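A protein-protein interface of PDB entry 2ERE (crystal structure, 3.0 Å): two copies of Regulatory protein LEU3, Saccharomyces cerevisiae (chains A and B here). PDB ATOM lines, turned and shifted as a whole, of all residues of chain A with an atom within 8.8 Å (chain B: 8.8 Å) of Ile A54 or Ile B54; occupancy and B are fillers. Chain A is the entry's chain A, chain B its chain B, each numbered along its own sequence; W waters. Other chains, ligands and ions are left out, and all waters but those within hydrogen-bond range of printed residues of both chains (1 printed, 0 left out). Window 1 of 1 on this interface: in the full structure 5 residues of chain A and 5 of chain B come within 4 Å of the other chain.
Ile B54 touches two residues of chain A. No residue of chain B comes within 4 Å of Ala A53. No residue of chain A comes within 4 Å of Ala B53. Of the printed residues of chain B, Glu A55 touches Arg B50 (3.1 Å) and Ile B54 (3.4 Å). Of the printed residues of chain A, Phe B58 touches Phe A58. Arg A48 touches none of the printed residues of chain B. The nearest residue of chain A that does not touch Ile B54 is Phe A58 (4.4 Å).
Asn A51 touches Asn B51. Ile A54 touches Ile B54. Ile A54 touches Glu B55 (CD1 to CG, 3.4 Å). CG of Glu A55 touches CD1 of Ile B54, 3.4 Å away. Phe A58 touches Phe B58 (CD1 to CD1, 3.5 Å).
OE1 of Glu A55 lies within salt-bridge range of NH2 of Arg B50, 3.1 Å away. OE1 of Glu B55 lies within salt-bridge range of NH2 of Arg A50 (3.1 Å).
Of the 16 printed residues of chain B, 5 touch a printed residue of chain A. Printed residues of chain B that touch a printed residue of chain A: Arg B50, Asn B51, Ile B54, Glu B55 and Phe B58. Hydrophobic or aromatic side chains of chain B that line the printed part of chain A: Ile B54 and Phe B58. Along chain B the printed residues that touch a printed residue of chain A span positions 50 to 58. Of the 16 printed residues of chain A, 5 touch a printed residue of chain B. Hydrophobic or aromatic side chains of chain A that line the printed part of chain B: Ile A54 and Phe A58. Among the printed residues, 7 pairs touch across the chains. Among the printed residues, Asp or Glu carboxylates within 4 Å of a Lys or Arg side-chain nitrogen of the other chain: Arg A50 with Glu B55 (3.1 Å) and Glu A55 with Arg B50 (3.1 Å).
Asn A51 touches its own counterpart, Asn B51. Ile B54 touches its own counterpart, Ile A54. Ile A54 touches Glu B55, and with the chains exchanged Glu A55 touches Ile B54. Phe A58 touches its own counterpart, Phe B58. Of the 7 pairs that touch across the chains among the printed residues, 7 have their exchanged pair printed and touching as well.
Water W1 lies within hydrogen-bond range of the side-chain amide nitrogen of Asn A51 (2.9 Å) and the side-chain amide nitrogen of Asn B51 (3.2 Å).
The backbone carbonyl oxygen (O) of Lys B47 sits close to the side-chain amide oxygen (OD1) of Asn B51 (2.6 Å). O of Lys A47 lies close to OD1 of Asn A51.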
ATOM      1  N   THR A  45      -1.630 -21.721  19.295  1.00  0.00           N
ATOM      2  CA  THR A  45      -2.346 -20.471  19.147  1.00  0.00           C
ATOM      3  C   THR A  45      -3.463 -20.452  20.153  1.00  0.00           C
ATOM      4  O   THR A  45      -4.187 -21.425  20.321  1.00  0.00           O
ATOM      5  CB  THR A  45      -2.971 -20.322  17.748  1.00  0.00           C
ATOM      6  OG1 THR A  45      -1.953 -19.950  16.813  1.00  0.00           O
ATOM      7  CG2 THR A  45      -4.069 -19.265  17.754  1.00  0.00           C
ATOM      8  N   LYS A  47      -6.476 -19.702  20.339  1.00  0.00           N
ATOM      9  CA  LYS A  47      -7.682 -19.496  19.557  1.00  0.00           C
ATOM     10  C   LYS A  47      -8.670 -18.497  20.171  1.00  0.00           C
ATOM     11  O   LYS A  47      -8.872 -17.403  19.649  1.00  0.00           O
ATOM     12  CB  LYS A  47      -8.389 -20.840  19.368  1.00  0.00           C
ATOM     13  CG  LYS A  47      -7.544 -21.943  18.756  1.00  0.00           C
ATOM     14  CD  LYS A  47      -7.448 -21.794  17.255  1.00  0.00           C
ATOM     15  CE  LYS A  47      -6.764 -22.997  16.634  1.00  0.00           C
ATOM     16  NZ  LYS A  47      -7.464 -24.268  16.967  1.00  0.00           N
ATOM     17  N   ARG A  48      -9.298 -18.899  21.267  1.00  0.00           N
ATOM     18  CA  ARG A  48     -10.273 -18.078  21.945  1.00  0.00           C
ATOM     19  C   ARG A  48      -9.867 -16.619  21.940  1.00  0.00           C
ATOM     20  O   ARG A  48     -10.305 -15.846  21.092  1.00  0.00           O
ATOM     21  CB  ARG A  48     -10.420 -18.551  23.376  1.00  0.00           C
ATOM     22  CG  ARG A  48     -11.839 -18.580  23.849  1.00  0.00           C
ATOM     23  CD  ARG A  48     -12.419 -19.967  23.690  1.00  0.00           C
ATOM     24  NE  ARG A  48     -11.922 -20.889  24.704  1.00  0.00           N
ATOM     25  CZ  ARG A  48     -12.289 -22.162  24.783  1.00  0.00           C
ATOM     26  NH1 ARG A  48     -13.152 -22.660  23.904  1.00  0.00           N
ATOM     27  NH2 ARG A  48     -11.811 -22.934  25.746  1.00  0.00           N
ATOM     28  N   ALA A  49      -9.028 -16.255  22.905  1.00  0.00           N
ATOM     29  CA  ALA A  49      -8.541 -14.890  23.053  1.00  0.00           C
ATOM     30  C   ALA A  49      -8.235 -14.269  21.697  1.00  0.00           C
ATOM     31  O   ALA A  49      -8.646 -13.147  21.392  1.00  0.00           O
ATOM     32  CB  ALA A  49      -7.296 -14.890  23.920  1.00  0.00           C
ATOM     33  N   ARG A  50      -7.508 -15.014  20.882  1.00  0.00           N
ATOM     34  CA  ARG A  50      -7.138 -14.551  19.560  1.00  0.00           C
ATOM     35  C   ARG A  50      -8.335 -14.020  18.788  1.00  0.00           C
ATOM     36  O   ARG A  50      -8.464 -12.823  18.535  1.00  0.00           O
ATOM     37  CB  ARG A  50      -6.496 -15.697  18.794  1.00  0.00           C
ATOM     38  CG  ARG A  50      -6.138 -15.358  17.377  1.00  0.00           C
ATOM     39  CD  ARG A  50      -7.307 -15.567  16.450  1.00  0.00           C
ATOM     40  NE  ARG A  50      -6.906 -15.360  15.066  1.00  0.00           N
ATOM     41  CZ  ARG A  50      -5.878 -15.977  14.489  1.00  0.00           C
ATOM     42  NH1 ARG A  50      -5.142 -16.843  15.177  1.00  0.00           N
ATOM     43  NH2 ARG A  50      -5.586 -15.728  13.220  1.00  0.00           N
ATOM     44  N   ASN A  51      -9.220 -14.925  18.416  1.00  0.00           N
ATOM     45  CA  ASN A  51     -10.389 -14.539  17.670  1.00  0.00           C
ATOM     46  C   ASN A  51     -11.085 -13.409  18.375  1.00  0.00           C
ATOM     47  O   ASN A  51     -11.744 -12.602  17.738  1.00  0.00           O
ATOM     48  CB  ASN A  51     -11.309 -15.728  17.510  1.00  0.00           C
ATOM     49  CG  ASN A  51     -10.655 -16.843  16.725  1.00  0.00           C
ATOM     50  OD1 ASN A  51      -9.742 -17.514  17.211  1.00  0.00           O
ATOM     51  ND2 ASN A  51     -11.099 -17.029  15.487  1.00  0.00           N
ATOM     52  N   GLU A  52     -10.928 -13.330  19.688  1.00  0.00           N
ATOM     53  CA  GLU A  52     -11.544 -12.239  20.418  1.00  0.00           C
ATOM     54  C   GLU A  52     -10.946 -10.937  19.919  1.00  0.00           C
ATOM     55  O   GLU A  52     -11.667  -9.991  19.602  1.00  0.00           O
ATOM     56  CB  GLU A  52     -11.298 -12.374  21.919  1.00  0.00           C
ATOM     57  CG  GLU A  52     -12.075 -13.499  22.590  1.00  0.00           C
ATOM     58  CD  GLU A  52     -12.711 -13.064  23.913  1.00  0.00           C
ATOM     59  OE1 GLU A  52     -13.357 -13.906  24.582  1.00  0.00           O
ATOM     60  OE2 GLU A  52     -12.567 -11.875  24.281  1.00  0.00           O
ATOM     61  N   ALA A  53      -9.620 -10.900  19.849  1.00  0.00           N
ATOM     62  CA  ALA A  53      -8.919  -9.713  19.379  1.00  0.00           C
ATOM     63  C   ALA A  53      -9.457  -9.370  18.005  1.00  0.00           C
ATOM     64  O   ALA A  53      -9.981  -8.278  17.782  1.00  0.00           O
ATOM     65  CB  ALA A  53      -7.423  -9.980  19.300  1.00  0.00           C
ATOM     66  N   ILE A  54      -9.332 -10.328  17.091  1.00  0.00           N
ATOM     67  CA  ILE A  54      -9.810 -10.157  15.732  1.00  0.00           C
ATOM     68  C   ILE A  54     -11.172  -9.491  15.708  1.00  0.00           C
ATOM     69  O   ILE A  54     -11.325  -8.399  15.170  1.00  0.00           O
ATOM     70  CB  ILE A  54      -9.925 -11.508  14.993  1.00  0.00           C
ATOM     71  CG1 ILE A  54      -8.550 -11.983  14.541  1.00  0.00           C
ATOM     72  CG2 ILE A  54     -10.825 -11.372  13.788  1.00  0.00           C
ATOM     73  CD1 ILE A  54      -8.603 -13.117  13.543  1.00  0.00           C
ATOM     74  N   GLU A  55     -12.160 -10.143  16.304  1.00  0.00           N
ATOM     75  CA  GLU A  55     -13.504  -9.599  16.302  1.00  0.00           C
ATOM     76  C   GLU A  55     -13.565  -8.196  16.865  1.00  0.00           C
ATOM     77  O   GLU A  55     -14.370  -7.381  16.424  1.00  0.00           O
ATOM     78  CB  GLU A  55     -14.450 -10.492  17.083  1.00  0.00           C
ATOM     79  CG  GLU A  55     -15.898 -10.157  16.824  1.00  0.00           C
ATOM     80  CD  GLU A  55     -16.836 -10.958  17.690  1.00  0.00           C
ATOM     81  OE1 GLU A  55     -16.796 -12.209  17.619  1.00  0.00           O
ATOM     82  OE2 GLU A  55     -17.612 -10.333  18.443  1.00  0.00           O
ATOM     83  N   LYS A  56     -12.718  -7.913  17.845  1.00  0.00           N
ATOM     84  CA  LYS A  56     -12.706  -6.585  18.429  1.00  0.00           C
ATOM     85  C   LYS A  56     -12.157  -5.601  17.404  1.00  0.00           C
ATOM     86  O   LYS A  56     -12.785  -4.585  17.109  1.00  0.00           O
ATOM     87  CB  LYS A  56     -11.855  -6.559  19.697  1.00  0.00           C
ATOM     88  CG  LYS A  56     -11.693  -5.164  20.286  1.00  0.00           C
ATOM     89  CD  LYS A  56     -10.867  -5.175  21.569  1.00  0.00           C
ATOM     90  CE  LYS A  56     -10.307  -3.784  21.914  1.00  0.00           C
ATOM     91  NZ  LYS A  56      -9.243  -3.314  20.958  1.00  0.00           N
ATOM     92  N   ARG A  57     -10.991  -5.910  16.851  1.00  0.00           N
ATOM     93  CA  ARG A  57     -10.374  -5.043  15.851  1.00  0.00           C
ATOM     94  C   ARG A  57     -11.284  -4.896  14.645  1.00  0.00           C
ATOM     95  O   ARG A  57     -11.422  -3.819  14.069  1.00  0.00           O
ATOM     96  CB  ARG A  57      -9.027  -5.618  15.420  1.00  0.00           C
ATOM     97  CG  ARG A  57      -8.044  -5.725  16.570  1.00  0.00           C
ATOM     98  CD  ARG A  57      -6.657  -6.105  16.095  1.00  0.00           C
ATOM     99  NE  ARG A  57      -6.596  -7.483  15.623  1.00  0.00           N
ATOM    100  CZ  ARG A  57      -5.464  -8.116  15.316  1.00  0.00           C
ATOM    101  NH1 ARG A  57      -4.295  -7.489  15.433  1.00  0.00           N
ATOM    102  NH2 ARG A  57      -5.496  -9.381  14.903  1.00  0.00           N
ATOM    103  N   PHE A  58     -11.905  -5.999  14.269  1.00  0.00           N
ATOM    104  CA  PHE A  58     -12.814  -6.003  13.146  1.00  0.00           C
ATOM    105  C   PHE A  58     -13.888  -4.970  13.417  1.00  0.00           C
ATOM    106  O   PHE A  58     -14.260  -4.204  12.539  1.00  0.00           O
ATOM    107  CB  PHE A  58     -13.451  -7.383  13.010  1.00  0.00           C
ATOM    108  CG  PHE A  58     -14.350  -7.531  11.815  1.00  0.00           C
ATOM    109  CD1 PHE A  58     -13.823  -7.577  10.528  1.00  0.00           C
ATOM    110  CD2 PHE A  58     -15.727  -7.656  11.981  1.00  0.00           C
ATOM    111  CE1 PHE A  58     -14.655  -7.746   9.417  1.00  0.00           C
ATOM    112  CE2 PHE A  58     -16.569  -7.826  10.880  1.00  0.00           C
ATOM    113  CZ  PHE A  58     -16.030  -7.872   9.593  1.00  0.00           C
ATOM    114  N   LYS A  59     -14.380  -4.945  14.648  1.00  0.00           N
ATOM    115  CA  LYS A  59     -15.426  -4.005  15.013  1.00  0.00           C
ATOM    116  C   LYS A  59     -14.988  -2.574  14.770  1.00  0.00           C
ATOM    117  O   LYS A  59     -15.646  -1.840  14.040  1.00  0.00           O
ATOM    118  CB  LYS A  59     -15.821  -4.190  16.470  1.00  0.00           C
ATOM    119  N   GLU A  60     -13.879  -2.177  15.384  1.00  0.00           N
ATOM    120  CA  GLU A  60     -13.379  -0.818  15.221  1.00  0.00           C
ATOM    121  C   GLU A  60     -13.526  -0.394  13.771  1.00  0.00           C
ATOM    122  O   GLU A  60     -13.922   0.735  13.478  1.00  0.00           O
ATOM    123  CB  GLU A  60     -11.925  -0.737  15.640  1.00  0.00           C
ATOM    124  N   LEU A  61     -13.217  -1.310  12.863  1.00  0.00           N
ATOM    125  CA  LEU A  61     -13.319  -1.023  11.444  1.00  0.00           C
ATOM    126  C   LEU A  61     -14.683  -0.435  11.071  1.00  0.00           C
ATOM    127  O   LEU A  61     -14.754   0.643  10.474  1.00  0.00           O
ATOM    128  CB  LEU A  61     -13.053  -2.283  10.651  1.00  0.00           C
ATOM    129  N   THR B  45     -24.761 -19.790  19.208  1.00  0.00           N
ATOM    130  CA  THR B  45     -23.891 -19.261  18.178  1.00  0.00           C
ATOM    131  C   THR B  45     -22.866 -20.304  17.845  1.00  0.00           C
ATOM    132  O   THR B  45     -22.282 -20.915  18.726  1.00  0.00           O
ATOM    133  CB  THR B  45     -23.141 -18.003  18.640  1.00  0.00           C
ATOM    134  OG1 THR B  45     -24.033 -16.886  18.597  1.00  0.00           O
ATOM    135  CG2 THR B  45     -21.933 -17.734  17.742  1.00  0.00           C
ATOM    136  N   LYS B  47     -19.816 -20.536  17.302  1.00  0.00           N
ATOM    137  CA  LYS B  47     -18.534 -19.887  17.511  1.00  0.00           C
ATOM    138  C   LYS B  47     -17.491 -20.187  16.432  1.00  0.00           C
ATOM    139  O   LYS B  47     -17.120 -19.311  15.653  1.00  0.00           O
ATOM    140  CB  LYS B  47     -17.973 -20.310  18.873  1.00  0.00           C
ATOM    141  CG  LYS B  47     -18.886 -20.071  20.071  1.00  0.00           C
ATOM    142  CD  LYS B  47     -18.841 -18.632  20.518  1.00  0.00           C
ATOM    143  CE  LYS B  47     -19.608 -18.443  21.812  1.00  0.00           C
ATOM    144  NZ  LYS B  47     -19.097 -19.326  22.893  1.00  0.00           N
ATOM    145  N   ARG B  48     -17.009 -21.423  16.415  1.00  0.00           N
ATOM    146  CA  ARG B  48     -16.001 -21.848  15.473  1.00  0.00           C
ATOM    147  C   ARG B  48     -16.233 -21.238  14.110  1.00  0.00           C
ATOM    148  O   ARG B  48     -15.643 -20.216  13.769  1.00  0.00           O
ATOM    149  CB  ARG B  48     -16.024 -23.361  15.352  1.00  0.00           C
ATOM    150  CG  ARG B  48     -14.654 -23.975  15.296  1.00  0.00           C
ATOM    151  CD  ARG B  48     -14.220 -24.436  16.671  1.00  0.00           C
ATOM    152  NE  ARG B  48     -14.897 -25.664  17.080  1.00  0.00           N
ATOM    153  CZ  ARG B  48     -14.688 -26.266  18.246  1.00  0.00           C
ATOM    154  NH1 ARG B  48     -13.824 -25.753  19.115  1.00  0.00           N
ATOM    155  NH2 ARG B  48     -15.330 -27.385  18.543  1.00  0.00           N
ATOM    156  N   ALA B  49     -17.101 -21.881  13.335  1.00  0.00           N
ATOM    157  CA  ALA B  49     -17.436 -21.432  11.990  1.00  0.00           C
ATOM    158  C   ALA B  49     -17.559 -19.912  11.926  1.00  0.00           C
ATOM    159  O   ALA B  49     -17.001 -19.254  11.044  1.00  0.00           O
ATOM    160  CB  ALA B  49     -18.740 -22.078  11.553  1.00  0.00           C
ATOM    161  N   ARG B  50     -18.298 -19.364  12.874  1.00  0.00           N
ATOM    162  CA  ARG B  50     -18.504 -17.933  12.942  1.00  0.00           C
ATOM    163  C   ARG B  50     -17.197 -17.166  12.846  1.00  0.00           C
ATOM    164  O   ARG B  50     -16.918 -16.488  11.860  1.00  0.00           O
ATOM    165  CB  ARG B  50     -19.210 -17.597  14.247  1.00  0.00           C
ATOM    166  CG  ARG B  50     -19.410 -16.128  14.468  1.00  0.00           C
ATOM    167  CD  ARG B  50     -18.203 -15.499  15.107  1.00  0.00           C
ATOM    168  NE  ARG B  50     -18.464 -14.105  15.425  1.00  0.00           N
ATOM    169  CZ  ARG B  50     -19.509 -13.691  16.136  1.00  0.00           C
ATOM    170  NH1 ARG B  50     -20.390 -14.570  16.601  1.00  0.00           N
ATOM    171  NH2 ARG B  50     -19.673 -12.398  16.384  1.00  0.00           N
ATOM    172  N   ASN B  51     -16.393 -17.277  13.890  1.00  0.00           N
ATOM    173  CA  ASN B  51     -15.127 -16.588  13.921  1.00  0.00           C
ATOM    174  C   ASN B  51     -14.360 -16.881  12.659  1.00  0.00           C
ATOM    175  O   ASN B  51     -13.560 -16.064  12.220  1.00  0.00           O
ATOM    176  CB  ASN B  51     -14.345 -17.013  15.145  1.00  0.00           C
ATOM    177  CG  ASN B  51     -15.056 -16.642  16.425  1.00  0.00           C
ATOM    178  OD1 ASN B  51     -16.075 -17.238  16.779  1.00  0.00           O
ATOM    179  ND2 ASN B  51     -14.541 -15.629  17.113  1.00  0.00           N
ATOM    180  N   GLU B  52     -14.607 -18.040  12.060  1.00  0.00           N
ATOM    181  CA  GLU B  52     -13.927 -18.364  10.816  1.00  0.00           C
ATOM    182  C   GLU B  52     -14.334 -17.331   9.771  1.00  0.00           C
ATOM    183  O   GLU B  52     -13.487 -16.756   9.083  1.00  0.00           O
ATOM    184  CB  GLU B  52     -14.308 -19.761  10.332  1.00  0.00           C
ATOM    185  CG  GLU B  52     -13.726 -20.897  11.160  1.00  0.00           C
ATOM    186  CD  GLU B  52     -13.156 -22.015  10.292  1.00  0.00           C
ATOM    187  OE1 GLU B  52     -12.669 -23.026  10.852  1.00  0.00           O
ATOM    188  OE2 GLU B  52     -13.193 -21.879   9.047  1.00  0.00           O
ATOM    189  N   ALA B  53     -15.639 -17.100   9.663  1.00  0.00           N
ATOM    190  CA  ALA B  53     -16.160 -16.130   8.712  1.00  0.00           C
ATOM    191  C   ALA B  53     -15.473 -14.809   8.986  1.00  0.00           C
ATOM    192  O   ALA B  53     -14.806 -14.251   8.117  1.00  0.00           O
ATOM    193  CB  ALA B  53     -17.663 -15.984   8.882  1.00  0.00           C
ATOM    194  N   ILE B  54     -15.638 -14.323  10.211  1.00  0.00           N
ATOM    195  CA  ILE B  54     -15.036 -13.070  10.623  1.00  0.00           C
ATOM    196  C   ILE B  54     -13.605 -12.949  10.127  1.00  0.00           C
ATOM    197  O   ILE B  54     -13.279 -12.046   9.363  1.00  0.00           O
ATOM    198  CB  ILE B  54     -15.022 -12.928  12.163  1.00  0.00           C
ATOM    199  CG1 ILE B  54     -16.401 -12.534  12.676  1.00  0.00           C
ATOM    200  CG2 ILE B  54     -14.018 -11.880  12.578  1.00  0.00           C
ATOM    201  CD1 ILE B  54     -16.400 -12.058  14.109  1.00  0.00           C
ATOM    202  N   GLU B  55     -12.752 -13.865  10.561  1.00  0.00           N
ATOM    203  CA  GLU B  55     -11.358 -13.809  10.170  1.00  0.00           C
ATOM    204  C   GLU B  55     -11.181 -13.794   8.669  1.00  0.00           C
ATOM    205  O   GLU B  55     -10.256 -13.164   8.160  1.00  0.00           O
ATOM    206  CB  GLU B  55     -10.590 -14.983  10.751  1.00  0.00           C
ATOM    207  CG  GLU B  55      -9.095 -14.792  10.659  1.00  0.00           C
ATOM    208  CD  GLU B  55      -8.325 -16.007  11.129  1.00  0.00           C
ATOM    209  OE1 GLU B  55      -8.497 -16.417  12.300  1.00  0.00           O
ATOM    210  OE2 GLU B  55      -7.543 -16.553  10.321  1.00  0.00           O
ATOM    211  N   LYS B  56     -12.061 -14.489   7.957  1.00  0.00           N
ATOM    212  CA  LYS B  56     -11.964 -14.517   6.508  1.00  0.00           C
ATOM    213  C   LYS B  56     -12.309 -13.138   5.966  1.00  0.00           C
ATOM    214  O   LYS B  56     -11.545 -12.557   5.197  1.00  0.00           O
ATOM    215  CB  LYS B  56     -12.905 -15.566   5.923  1.00  0.00           C
ATOM    216  CG  LYS B  56     -12.950 -15.547   4.403  1.00  0.00           C
ATOM    217  CD  LYS B  56     -13.876 -16.627   3.850  1.00  0.00           C
ATOM    218  CE  LYS B  56     -14.297 -16.340   2.398  1.00  0.00           C
ATOM    219  NZ  LYS B  56     -15.217 -15.158   2.269  1.00  0.00           N
ATOM    220  N   ARG B  57     -13.455 -12.610   6.382  1.00  0.00           N
ATOM    221  CA  ARG B  57     -13.887 -11.287   5.937  1.00  0.00           C
ATOM    222  C   ARG B  57     -12.872 -10.234   6.350  1.00  0.00           C
ATOM    223  O   ARG B  57     -12.563  -9.309   5.601  1.00  0.00           O
ATOM    224  CB  ARG B  57     -15.256 -10.953   6.531  1.00  0.00           C
ATOM    225  CG  ARG B  57     -16.341 -11.924   6.097  1.00  0.00           C
ATOM    226  CD  ARG B  57     -17.719 -11.466   6.533  1.00  0.00           C
ATOM    227  NE  ARG B  57     -17.901 -11.552   7.981  1.00  0.00           N
ATOM    228  CZ  ARG B  57     -19.071 -11.379   8.599  1.00  0.00           C
ATOM    229  NH1 ARG B  57     -20.170 -11.108   7.892  1.00  0.00           N
ATOM    230  NH2 ARG B  57     -19.151 -11.488   9.924  1.00  0.00           N
ATOM    231  N   PHE B  58     -12.359 -10.388   7.558  1.00  0.00           N
ATOM    232  CA  PHE B  58     -11.371  -9.472   8.074  1.00  0.00           C
ATOM    233  C   PHE B  58     -10.210  -9.449   7.100  1.00  0.00           C
ATOM    234  O   PHE B  58      -9.683  -8.390   6.777  1.00  0.00           O
ATOM    235  CB  PHE B  58     -10.891  -9.952   9.437  1.00  0.00           C
ATOM    236  CG  PHE B  58      -9.922  -9.021  10.104  1.00  0.00           C
ATOM    237  CD1 PHE B  58     -10.345  -7.794  10.609  1.00  0.00           C
ATOM    238  CD2 PHE B  58      -8.586  -9.383  10.255  1.00  0.00           C
ATOM    239  CE1 PHE B  58      -9.451  -6.938  11.262  1.00  0.00           C
ATOM    240  CE2 PHE B  58      -7.682  -8.539  10.905  1.00  0.00           C
ATOM    241  CZ  PHE B  58      -8.117  -7.312  11.410  1.00  0.00           C
ATOM    242  N   LYS B  59      -9.819 -10.626   6.625  1.00  0.00           N
ATOM    243  CA  LYS B  59      -8.704 -10.728   5.693  1.00  0.00           C
ATOM    244  C   LYS B  59      -8.947  -9.902   4.443  1.00  0.00           C
ATOM    245  O   LYS B  59      -8.147  -9.032   4.107  1.00  0.00           O
ATOM    246  CB  LYS B  59      -8.455 -12.179   5.312  1.00  0.00           C
ATOM    247  N   GLU B  60     -10.049 -10.176   3.754  1.00  0.00           N
ATOM    248  CA  GLU B  60     -10.376  -9.442   2.536  1.00  0.00           C
ATOM    249  C   GLU B  60     -10.064  -7.966   2.731  1.00  0.00           C
ATOM    250  O   GLU B  60      -9.517  -7.313   1.842  1.00  0.00           O
ATOM    251  CB  GLU B  60     -11.845  -9.622   2.191  1.00  0.00           C
ATOM    252  N   LEU B  61     -10.405  -7.448   3.905  1.00  0.00           N
ATOM    253  CA  LEU B  61     -10.157  -6.049   4.209  1.00  0.00           C
ATOM    254  C   LEU B  61      -8.706  -5.644   3.919  1.00  0.00           C
ATOM    255  O   LEU B  61      -8.462  -4.695   3.173  1.00  0.00           O
ATOM    256  CB  LEU B  61     -10.503  -5.774   5.657  1.00  0.00           C
HETATM  257  O   HOH W   1     -12.426 -14.550  14.957  1.00  0.00           O
